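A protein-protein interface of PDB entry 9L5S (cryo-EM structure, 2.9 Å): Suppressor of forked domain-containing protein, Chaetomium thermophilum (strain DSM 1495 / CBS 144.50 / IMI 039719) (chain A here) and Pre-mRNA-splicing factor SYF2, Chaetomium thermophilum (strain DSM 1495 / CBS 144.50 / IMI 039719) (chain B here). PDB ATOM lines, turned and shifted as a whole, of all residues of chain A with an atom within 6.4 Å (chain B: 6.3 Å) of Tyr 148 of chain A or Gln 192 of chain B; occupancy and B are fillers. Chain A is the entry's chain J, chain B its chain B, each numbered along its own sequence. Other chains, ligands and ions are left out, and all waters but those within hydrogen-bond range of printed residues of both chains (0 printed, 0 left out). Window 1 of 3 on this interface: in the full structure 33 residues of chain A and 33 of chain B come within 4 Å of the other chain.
Tyr 148 of chain A touches two residues of chain B. Of the printed residues of chain B, Val 147 of chain A touches Tyr 189 (3.8 Å). Of the printed residues of chain B, Met 152 of chain A touches Met 196 (3.6 Å), Arg 261 (3.2 Å), Leu 262 (3.6 Å) and Asp 265 (3.8 Å). Of the printed residues of chain B, Glu 151 of chain A touches Tyr 189 (3.7 Å) and Ile 193 (3.6 Å). Printed residues of chain A within 4 Å of Thr 188 of chain B: Lys 141 (3.5 Å). Of the printed residues of chain A, Arg 261 of chain B touches Met 152 (3.2 Å). Arg 194 of chain B touches none of the printed residues of chain A. The nearest residue of chain B that does not touch Tyr 148 of chain A is Tyr 189 of chain B (4.1 Å). The nearest residue of chain A that does not touch Gln 192 of chain B is Tyr 144 of chain A (5.5 Å).
O of Met 152 of chain A is in hydrogen-bond range of NH2 of Arg 261 of chain B (3.2 Å). The side-chain hydroxyl (OH) of Tyr 148 of chain A lies close to the side-chain carboxylate (OD2) of Asp 265 of chain B, 2.3 Å away.
Among the printed residues, pairs that only touch across the chains: Tyr 144 of chain A with Tyr 189 of chain B (3.4 Å), Tyr 148 of chain A with Gln 192 of chain B (3.5 Å), Lys 141 of chain A with Thr 188 of chain B (3.5 Å), Met 152 of chain A with Leu 262 of chain B (3.6 Å), Met 152 of chain A with Met 196 of chain B (3.6 Å), Glu 151 of chain A with Ile 193 of chain B (3.6 Å), Glu 151 of chain A with Tyr 189 of chain B (3.7 Å), Leu 153 of chain A with Leu 262 of chain B (3.8 Å), Met 152 of chain A with Asp 265 of chain B (3.8 Å), Val 147 of chain A with Tyr 189 of chain B (3.8 Å), Lys 145 of chain A with Leu 266 of chain B (3.97 Å) and Val 149 of chain A with Leu 262 of chain B (3.99 Å).
The backbone NH of Glu 151 of chain A is in hydrogen-bond range of the side-chain hydroxyl of Thr 159 of chain A (3.5 Å).
Printed residues of chain A that touch a printed residue of chain B: Lys 141, Tyr 144, Lys 145, Val 147, Tyr 148, Val 149, Glu 151, Met 152 and Leu 153. Of the 15 printed residues of chain B, 9 touch a printed residue of chain A. Printed residues of chain B that touch a printed residue of chain A: Thr 188, Tyr 189, Gln 192, Ile 193, Met 196, Arg 261, Leu 262, Asp 265 and Leu 266. Hydrophobic or aromatic side chains of chain B that line the printed part of chain A: Tyr 189, Ile 193, Met 196, Leu 262 and Leu 266.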
ATOM      1  N   LYS A 141     -19.185 -33.247  27.388  1.00  0.00           N
ATOM      2  CA  LYS A 141     -18.196 -32.254  27.798  1.00  0.00           C
ATOM      3  C   LYS A 141     -16.805 -32.611  27.288  1.00  0.00           C
ATOM      4  O   LYS A 141     -16.075 -31.744  26.791  1.00  0.00           O
ATOM      5  CB  LYS A 141     -18.193 -32.131  29.322  1.00  0.00           C
ATOM      6  CG  LYS A 141     -17.209 -31.117  29.876  1.00  0.00           C
ATOM      7  CD  LYS A 141     -17.785 -29.715  29.837  1.00  0.00           C
ATOM      8  CE  LYS A 141     -16.795 -28.696  30.375  1.00  0.00           C
ATOM      9  NZ  LYS A 141     -17.258 -27.304  30.128  1.00  0.00           N
ATOM     10  N   TRP A 143     -16.042 -34.618  24.685  1.00  0.00           N
ATOM     11  CA  TRP A 143     -16.040 -34.493  23.231  1.00  0.00           C
ATOM     12  C   TRP A 143     -15.961 -33.033  22.798  1.00  0.00           C
ATOM     13  O   TRP A 143     -15.245 -32.700  21.846  1.00  0.00           O
ATOM     14  CB  TRP A 143     -17.296 -35.142  22.653  1.00  0.00           C
ATOM     15  CG  TRP A 143     -17.308 -36.638  22.678  1.00  0.00           C
ATOM     16  CD1 TRP A 143     -18.011 -37.436  23.531  1.00  0.00           C
ATOM     17  CD2 TRP A 143     -16.634 -37.518  21.770  1.00  0.00           C
ATOM     18  NE1 TRP A 143     -17.790 -38.758  23.234  1.00  0.00           N
ATOM     19  CE2 TRP A 143     -16.951 -38.835  22.154  1.00  0.00           C
ATOM     20  CE3 TRP A 143     -15.783 -37.318  20.681  1.00  0.00           C
ATOM     21  CZ2 TRP A 143     -16.447 -39.947  21.487  1.00  0.00           C
ATOM     22  CZ3 TRP A 143     -15.284 -38.423  20.019  1.00  0.00           C
ATOM     23  CH2 TRP A 143     -15.616 -39.721  20.424  1.00  0.00           C
ATOM     24  N   TYR A 144     -16.701 -32.154  23.482  1.00  0.00           N
ATOM     25  CA  TYR A 144     -16.686 -30.733  23.153  1.00  0.00           C
ATOM     26  C   TYR A 144     -15.318 -30.121  23.413  1.00  0.00           C
ATOM     27  O   TYR A 144     -14.817 -29.339  22.594  1.00  0.00           O
ATOM     28  CB  TYR A 144     -17.761 -29.995  23.952  1.00  0.00           C
ATOM     29  CG  TYR A 144     -19.100 -29.928  23.258  1.00  0.00           C
ATOM     30  CD1 TYR A 144     -19.191 -29.560  21.925  1.00  0.00           C
ATOM     31  CD2 TYR A 144     -20.275 -30.217  23.939  1.00  0.00           C
ATOM     32  CE1 TYR A 144     -20.411 -29.495  21.285  1.00  0.00           C
ATOM     33  CE2 TYR A 144     -21.500 -30.155  23.308  1.00  0.00           C
ATOM     34  CZ  TYR A 144     -21.561 -29.792  21.980  1.00  0.00           C
ATOM     35  OH  TYR A 144     -22.776 -29.725  21.344  1.00  0.00           O
ATOM     36  N   LYS A 145     -14.687 -30.484  24.534  1.00  0.00           N
ATOM     37  CA  LYS A 145     -13.323 -30.034  24.782  1.00  0.00           C
ATOM     38  C   LYS A 145     -12.365 -30.574  23.728  1.00  0.00           C
ATOM     39  O   LYS A 145     -11.465 -29.862  23.281  1.00  0.00           O
ATOM     40  CB  LYS A 145     -12.861 -30.447  26.181  1.00  0.00           C
ATOM     41  CG  LYS A 145     -11.413 -30.065  26.458  1.00  0.00           C
ATOM     42  CD  LYS A 145     -11.053 -30.098  27.922  1.00  0.00           C
ATOM     43  CE  LYS A 145     -11.107 -28.705  28.515  1.00  0.00           C
ATOM     44  NZ  LYS A 145      -9.858 -27.949  28.233  1.00  0.00           N
ATOM     45  N   TYR A 146     -12.572 -31.814  23.288  1.00  0.00           N
ATOM     46  CA  TYR A 146     -11.640 -32.434  22.352  1.00  0.00           C
ATOM     47  C   TYR A 146     -11.713 -31.770  20.976  1.00  0.00           C
ATOM     48  O   TYR A 146     -10.673 -31.458  20.373  1.00  0.00           O
ATOM     49  CB  TYR A 146     -11.936 -33.936  22.308  1.00  0.00           C
ATOM     50  CG  TYR A 146     -10.957 -34.809  21.563  1.00  0.00           C
ATOM     51  CD1 TYR A 146      -9.639 -34.424  21.389  1.00  0.00           C
ATOM     52  CD2 TYR A 146     -11.323 -36.084  21.150  1.00  0.00           C
ATOM     53  CE1 TYR A 146      -8.735 -35.247  20.755  1.00  0.00           C
ATOM     54  CE2 TYR A 146     -10.427 -36.911  20.504  1.00  0.00           C
ATOM     55  CZ  TYR A 146      -9.133 -36.486  20.308  1.00  0.00           C
ATOM     56  OH  TYR A 146      -8.228 -37.304  19.673  1.00  0.00           O
ATOM     57  N   VAL A 147     -12.928 -31.480  20.494  1.00  0.00           N
ATOM     58  CA  VAL A 147     -13.055 -30.777  19.218  1.00  0.00           C
ATOM     59  C   VAL A 147     -12.586 -29.331  19.351  1.00  0.00           C
ATOM     60  O   VAL A 147     -11.993 -28.776  18.419  1.00  0.00           O
ATOM     61  CB  VAL A 147     -14.489 -30.858  18.653  1.00  0.00           C
ATOM     62  CG1 VAL A 147     -14.800 -32.262  18.179  1.00  0.00           C
ATOM     63  CG2 VAL A 147     -15.533 -30.364  19.631  1.00  0.00           C
ATOM     64  N   TYR A 148     -12.822 -28.699  20.508  1.00  0.00           N
ATOM     65  CA  TYR A 148     -12.373 -27.322  20.698  1.00  0.00           C
ATOM     66  C   TYR A 148     -10.850 -27.227  20.712  1.00  0.00           C
ATOM     67  O   TYR A 148     -10.275 -26.304  20.123  1.00  0.00           O
ATOM     68  CB  TYR A 148     -12.963 -26.761  21.992  1.00  0.00           C
ATOM     69  CG  TYR A 148     -12.222 -25.569  22.544  1.00  0.00           C
ATOM     70  CD1 TYR A 148     -12.319 -24.326  21.931  1.00  0.00           C
ATOM     71  CD2 TYR A 148     -11.437 -25.682  23.683  1.00  0.00           C
ATOM     72  CE1 TYR A 148     -11.645 -23.231  22.433  1.00  0.00           C
ATOM     73  CE2 TYR A 148     -10.761 -24.594  24.191  1.00  0.00           C
ATOM     74  CZ  TYR A 148     -10.869 -23.373  23.565  1.00  0.00           C
ATOM     75  OH  TYR A 148     -10.192 -22.296  24.079  1.00  0.00           O
ATOM     76  N   VAL A 149     -10.185 -28.176  21.373  1.00  0.00           N
ATOM     77  CA  VAL A 149      -8.726 -28.184  21.422  1.00  0.00           C
ATOM     78  C   VAL A 149      -8.140 -28.466  20.044  1.00  0.00           C
ATOM     79  O   VAL A 149      -7.216 -27.776  19.600  1.00  0.00           O
ATOM     80  CB  VAL A 149      -8.223 -29.187  22.477  1.00  0.00           C
ATOM     81  CG1 VAL A 149      -6.717 -29.336  22.401  1.00  0.00           C
ATOM     82  CG2 VAL A 149      -8.584 -28.693  23.861  1.00  0.00           C
ATOM     83  N   MET A 150      -8.680 -29.455  19.325  1.00  0.00           N
ATOM     84  CA  MET A 150      -8.115 -29.678  17.998  1.00  0.00           C
ATOM     85  C   MET A 150      -8.675 -28.744  16.934  1.00  0.00           C
ATOM     86  O   MET A 150      -8.363 -28.935  15.755  1.00  0.00           O
ATOM     87  CB  MET A 150      -8.283 -31.129  17.541  1.00  0.00           C
ATOM     88  CG  MET A 150      -7.486 -32.129  18.349  1.00  0.00           C
ATOM     89  SD  MET A 150      -7.788 -33.811  17.794  1.00  0.00           S
ATOM     90  CE  MET A 150      -6.956 -33.790  16.212  1.00  0.00           C
ATOM     91  N   GLU A 151      -9.520 -27.778  17.293  1.00  0.00           N
ATOM     92  CA  GLU A 151      -9.777 -26.668  16.383  1.00  0.00           C
ATOM     93  C   GLU A 151      -8.894 -25.467  16.704  1.00  0.00           C
ATOM     94  O   GLU A 151      -8.474 -24.746  15.792  1.00  0.00           O
ATOM     95  CB  GLU A 151     -11.256 -26.269  16.425  1.00  0.00           C
ATOM     96  CG  GLU A 151     -11.625 -25.162  15.444  1.00  0.00           C
ATOM     97  CD  GLU A 151     -13.116 -24.920  15.356  1.00  0.00           C
ATOM     98  OE1 GLU A 151     -13.891 -25.758  15.861  1.00  0.00           O
ATOM     99  OE2 GLU A 151     -13.513 -23.888  14.776  1.00  0.00           O
ATOM    100  N   MET A 152      -8.594 -25.242  17.989  1.00  0.00           N
ATOM    101  CA  MET A 152      -7.662 -24.200  18.409  1.00  0.00           C
ATOM    102  C   MET A 152      -6.259 -24.386  17.840  1.00  0.00           C
ATOM    103  O   MET A 152      -5.586 -23.391  17.549  1.00  0.00           O
ATOM    104  CB  MET A 152      -7.584 -24.155  19.941  1.00  0.00           C
ATOM    105  CG  MET A 152      -6.728 -23.029  20.512  1.00  0.00           C
ATOM    106  SD  MET A 152      -7.272 -21.340  20.207  1.00  0.00           S
ATOM    107  CE  MET A 152      -8.677 -21.259  21.310  1.00  0.00           C
ATOM    108  N   LEU A 153      -5.819 -25.627  17.634  1.00  0.00           N
ATOM    109  CA  LEU A 153      -4.473 -25.924  17.160  1.00  0.00           C
ATOM    110  C   LEU A 153      -4.412 -26.082  15.644  1.00  0.00           C
ATOM    111  O   LEU A 153      -3.614 -26.878  15.138  1.00  0.00           O
ATOM    112  CB  LEU A 153      -3.941 -27.185  17.839  1.00  0.00           C
ATOM    113  CG  LEU A 153      -3.936 -27.217  19.366  1.00  0.00           C
ATOM    114  CD1 LEU A 153      -3.777 -28.643  19.857  1.00  0.00           C
ATOM    115  CD2 LEU A 153      -2.822 -26.341  19.901  1.00  0.00           C
ATOM    116  N   THR A 159     -10.062 -32.418  13.578  1.00  0.00           N
ATOM    117  CA  THR A 159     -11.336 -32.076  14.200  1.00  0.00           C
ATOM    118  C   THR A 159     -12.481 -32.788  13.494  1.00  0.00           C
ATOM    119  O   THR A 159     -13.439 -33.236  14.135  1.00  0.00           O
ATOM    120  CB  THR A 159     -11.546 -30.563  14.153  1.00  0.00           C
ATOM    121  OG1 THR A 159     -10.414 -29.916  14.735  1.00  0.00           O
ATOM    122  CG2 THR A 159     -12.771 -30.167  14.959  1.00  0.00           C
ATOM    123  N   LYS B 187     -23.235 -24.758  25.877  1.00  0.00           N
ATOM    124  CA  LYS B 187     -23.146 -23.313  26.072  1.00  0.00           C
ATOM    125  C   LYS B 187     -21.699 -22.831  26.035  1.00  0.00           C
ATOM    126  O   LYS B 187     -21.380 -21.849  25.352  1.00  0.00           O
ATOM    127  CB  LYS B 187     -23.807 -22.923  27.395  1.00  0.00           C
ATOM    128  CG  LYS B 187     -25.316 -22.738  27.311  1.00  0.00           C
ATOM    129  CD  LYS B 187     -25.999 -22.922  28.666  1.00  0.00           C
ATOM    130  CE  LYS B 187     -25.219 -22.270  29.801  1.00  0.00           C
ATOM    131  NZ  LYS B 187     -25.870 -22.487  31.121  1.00  0.00           N
ATOM    132  N   THR B 188     -20.805 -23.517  26.754  1.00  0.00           N
ATOM    133  CA  THR B 188     -19.399 -23.119  26.755  1.00  0.00           C
ATOM    134  C   THR B 188     -18.739 -23.369  25.406  1.00  0.00           C
ATOM    135  O   THR B 188     -17.855 -22.608  24.998  1.00  0.00           O
ATOM    136  CB  THR B 188     -18.626 -23.839  27.864  1.00  0.00           C
ATOM    137  OG1 THR B 188     -18.619 -25.252  27.618  1.00  0.00           O
ATOM    138  CG2 THR B 188     -19.212 -23.530  29.235  1.00  0.00           C
ATOM    139  N   TYR B 189     -19.154 -24.422  24.691  1.00  0.00           N
ATOM    140  CA  TYR B 189     -18.602 -24.645  23.358  1.00  0.00           C
ATOM    141  C   TYR B 189     -19.029 -23.548  22.391  1.00  0.00           C
ATOM    142  O   TYR B 189     -18.215 -23.071  21.593  1.00  0.00           O
ATOM    143  CB  TYR B 189     -19.018 -26.008  22.815  1.00  0.00           C
ATOM    144  CG  TYR B 189     -18.433 -26.284  21.449  1.00  0.00           C
ATOM    145  CD1 TYR B 189     -17.063 -26.445  21.284  1.00  0.00           C
ATOM    146  CD2 TYR B 189     -19.241 -26.356  20.322  1.00  0.00           C
ATOM    147  CE1 TYR B 189     -16.517 -26.689  20.040  1.00  0.00           C
ATOM    148  CE2 TYR B 189     -18.702 -26.600  19.074  1.00  0.00           C
ATOM    149  CZ  TYR B 189     -17.340 -26.765  18.939  1.00  0.00           C
ATOM    150  OH  TYR B 189     -16.801 -27.008  17.697  1.00  0.00           O
ATOM    151  N   LYS B 190     -20.300 -23.136  22.450  1.00  0.00           N
ATOM    152  CA  LYS B 190     -20.767 -22.036  21.612  1.00  0.00           C
ATOM    153  C   LYS B 190     -20.060 -20.736  21.970  1.00  0.00           C
ATOM    154  O   LYS B 190     -19.704 -19.947  21.087  1.00  0.00           O
ATOM    155  CB  LYS B 190     -22.283 -21.882  21.746  1.00  0.00           C
ATOM    156  CG  LYS B 190     -23.081 -22.724  20.766  1.00  0.00           C
ATOM    157  CD  LYS B 190     -24.484 -22.992  21.284  1.00  0.00           C
ATOM    158  CE  LYS B 190     -25.471 -23.129  20.138  1.00  0.00           C
ATOM    159  NZ  LYS B 190     -26.868 -23.314  20.619  1.00  0.00           N
ATOM    160  N   ARG B 191     -19.838 -20.504  23.268  1.00  0.00           N
ATOM    161  CA  ARG B 191     -19.118 -19.312  23.709  1.00  0.00           C
ATOM    162  C   ARG B 191     -17.677 -19.312  23.208  1.00  0.00           C
ATOM    163  O   ARG B 191     -17.164 -18.281  22.758  1.00  0.00           O
ATOM    164  CB  ARG B 191     -19.167 -19.221  25.234  1.00  0.00           C
ATOM    165  CG  ARG B 191     -18.581 -17.945  25.806  1.00  0.00           C
ATOM    166  CD  ARG B 191     -18.750 -17.906  27.314  1.00  0.00           C
ATOM    167  NE  ARG B 191     -18.426 -19.188  27.926  1.00  0.00           N
ATOM    168  CZ  ARG B 191     -17.232 -19.510  28.403  1.00  0.00           C
ATOM    169  NH1 ARG B 191     -16.216 -18.665  28.352  1.00  0.00           N
ATOM    170  NH2 ARG B 191     -17.052 -20.710  28.946  1.00  0.00           N
ATOM    171  N   GLN B 192     -17.011 -20.468  23.259  1.00  0.00           N
ATOM    172  CA  GLN B 192     -15.624 -20.549  22.808  1.00  0.00           C
ATOM    173  C   GLN B 192     -15.523 -20.420  21.291  1.00  0.00           C
ATOM    174  O   GLN B 192     -14.572 -19.821  20.773  1.00  0.00           O
ATOM    175  CB  GLN B 192     -15.002 -21.861  23.283  1.00  0.00           C
ATOM    176  CG  GLN B 192     -14.611 -21.859  24.754  1.00  0.00           C
ATOM    177  CD  GLN B 192     -14.381 -23.255  25.298  1.00  0.00           C
ATOM    178  OE1 GLN B 192     -14.702 -24.247  24.645  1.00  0.00           O
ATOM    179  NE2 GLN B 192     -13.824 -23.339  26.500  1.00  0.00           N
ATOM    180  N   ILE B 193     -16.491 -20.978  20.563  1.00  0.00           N
ATOM    181  CA  ILE B 193     -16.526 -20.824  19.111  1.00  0.00           C
ATOM    182  C   ILE B 193     -16.804 -19.370  18.732  1.00  0.00           C
ATOM    183  O   ILE B 193     -16.272 -18.858  17.741  1.00  0.00           O
ATOM    184  CB  ILE B 193     -17.555 -21.806  18.514  1.00  0.00           C
ATOM    185  CG1 ILE B 193     -17.019 -23.240  18.577  1.00  0.00           C
ATOM    186  CG2 ILE B 193     -17.921 -21.455  17.087  1.00  0.00           C
ATOM    187  CD1 ILE B 193     -15.602 -23.400  18.058  1.00  0.00           C
ATOM    188  N   ARG B 194     -17.627 -18.677  19.521  1.00  0.00           N
ATOM    189  CA  ARG B 194     -17.807 -17.243  19.317  1.00  0.00           C
ATOM    190  C   ARG B 194     -16.516 -16.478  19.598  1.00  0.00           C
ATOM    191  O   ARG B 194     -16.175 -15.533  18.877  1.00  0.00           O
ATOM    192  CB  ARG B 194     -18.953 -16.739  20.194  1.00  0.00           C
ATOM    193  CG  ARG B 194     -19.136 -15.232  20.205  1.00  0.00           C
ATOM    194  CD  ARG B 194     -20.001 -14.804  21.376  1.00  0.00           C
ATOM    195  NE  ARG B 194     -21.046 -15.783  21.650  1.00  0.00           N
ATOM    196  CZ  ARG B 194     -21.404 -16.180  22.862  1.00  0.00           C
ATOM    197  NH1 ARG B 194     -20.817 -15.703  23.947  1.00  0.00           N
ATOM    198  NH2 ARG B 194     -22.375 -17.080  22.990  1.00  0.00           N
ATOM    199  N   ASN B 195     -15.775 -16.886  20.632  1.00  0.00           N
ATOM    200  CA  ASN B 195     -14.501 -16.254  20.965  1.00  0.00           C
ATOM    201  C   ASN B 195     -13.366 -16.657  20.030  1.00  0.00           C
ATOM    202  O   ASN B 195     -12.268 -16.103  20.154  1.00  0.00           O
ATOM    203  CB  ASN B 195     -14.112 -16.570  22.412  1.00  0.00           C
ATOM    204  CG  ASN B 195     -15.122 -16.050  23.416  1.00  0.00           C
ATOM    205  OD1 ASN B 195     -15.744 -15.009  23.210  1.00  0.00           O
ATOM    206  ND2 ASN B 195     -15.289 -16.778  24.514  1.00  0.00           N
ATOM    207  N   MET B 196     -13.589 -17.627  19.137  1.00  0.00           N
ATOM    208  CA  MET B 196     -12.656 -17.861  18.037  1.00  0.00           C
ATOM    209  C   MET B 196     -12.461 -16.596  17.210  1.00  0.00           C
ATOM    210  O   MET B 196     -11.336 -16.247  16.837  1.00  0.00           O
ATOM    211  CB  MET B 196     -13.181 -18.970  17.125  1.00  0.00           C
ATOM    212  CG  MET B 196     -12.962 -20.406  17.555  1.00  0.00           C
ATOM    213  SD  MET B 196     -11.354 -21.060  17.073  1.00  0.00           S
ATOM    214  CE  MET B 196     -10.880 -21.954  18.542  1.00  0.00           C
ATOM    215  N   GLY B 197     -13.551 -15.897  16.921  1.00  0.00           N
ATOM    216  CA  GLY B 197     -13.543 -14.901  15.879  1.00  0.00           C
ATOM    217  C   GLY B 197     -13.825 -15.545  14.539  1.00  0.00           C
ATOM    218  O   GLY B 197     -14.204 -16.717  14.440  1.00  0.00           O
ATOM    219  N   ARG B 261      -1.948 -19.591  21.648  1.00  0.00           N
ATOM    220  CA  ARG B 261      -3.345 -19.184  21.778  1.00  0.00           C
ATOM    221  C   ARG B 261      -4.107 -20.098  22.730  1.00  0.00           C
ATOM    222  O   ARG B 261      -4.894 -19.625  23.559  1.00  0.00           O
ATOM    223  CB  ARG B 261      -4.016 -19.173  20.404  1.00  0.00           C
ATOM    224  CG  ARG B 261      -3.702 -17.952  19.559  1.00  0.00           C
ATOM    225  CD  ARG B 261      -4.618 -17.872  18.348  1.00  0.00           C
ATOM    226  NE  ARG B 261      -4.290 -18.885  17.352  1.00  0.00           N
ATOM    227  CZ  ARG B 261      -5.139 -19.800  16.902  1.00  0.00           C
ATOM    228  NH1 ARG B 261      -6.385 -19.863  17.341  1.00  0.00           N
ATOM    229  NH2 ARG B 261      -4.726 -20.674  15.989  1.00  0.00           N
ATOM    230  N   LEU B 262      -3.882 -21.411  22.624  1.00  0.00           N
ATOM    231  CA  LEU B 262      -4.557 -22.358  23.511  1.00  0.00           C
ATOM    232  C   LEU B 262      -4.130 -22.173  24.963  1.00  0.00           C
ATOM    233  O   LEU B 262      -4.977 -22.165  25.870  1.00  0.00           O
ATOM    234  CB  LEU B 262      -4.284 -23.788  23.051  1.00  0.00           C
ATOM    235  CG  LEU B 262      -4.935 -24.916  23.848  1.00  0.00           C
ATOM    236  CD1 LEU B 262      -6.446 -24.883  23.717  1.00  0.00           C
ATOM    237  CD2 LEU B 262      -4.400 -26.237  23.354  1.00  0.00           C
ATOM    238  N   ASP B 265      -5.685 -18.959  26.284  1.00  0.00           N
ATOM    239  CA  ASP B 265      -7.109 -19.083  26.588  1.00  0.00           C
ATOM    240  C   ASP B 265      -7.341 -19.888  27.865  1.00  0.00           C
ATOM    241  O   ASP B 265      -8.222 -19.548  28.668  1.00  0.00           O
ATOM    242  CB  ASP B 265      -7.846 -19.715  25.408  1.00  0.00           C
ATOM    243  CG  ASP B 265      -9.346 -19.493  25.471  1.00  0.00           C
ATOM    244  OD1 ASP B 265      -9.798 -18.704  26.328  1.00  0.00           O
ATOM    245  OD2 ASP B 265     -10.074 -20.099  24.659  1.00  0.00           O
ATOM    246  N   LEU B 266      -6.560 -20.955  28.072  1.00  0.00           N
ATOM    247  CA  LEU B 266      -6.675 -21.721  29.313  1.00  0.00           C
ATOM    248  C   LEU B 266      -6.279 -20.882  30.524  1.00  0.00           C
ATOM    249  O   LEU B 266      -6.940 -20.933  31.572  1.00  0.00           O
ATOM    250  CB  LEU B 266      -5.826 -22.990  29.231  1.00  0.00           C
ATOM    251  CG  LEU B 266      -6.315 -24.049  28.241  1.00  0.00           C
ATOM    252  CD1 LEU B 266      -5.204 -25.030  27.906  1.00  0.00           C
ATOM    253  CD2 LEU B 266      -7.529 -24.778  28.793  1.00  0.00           C
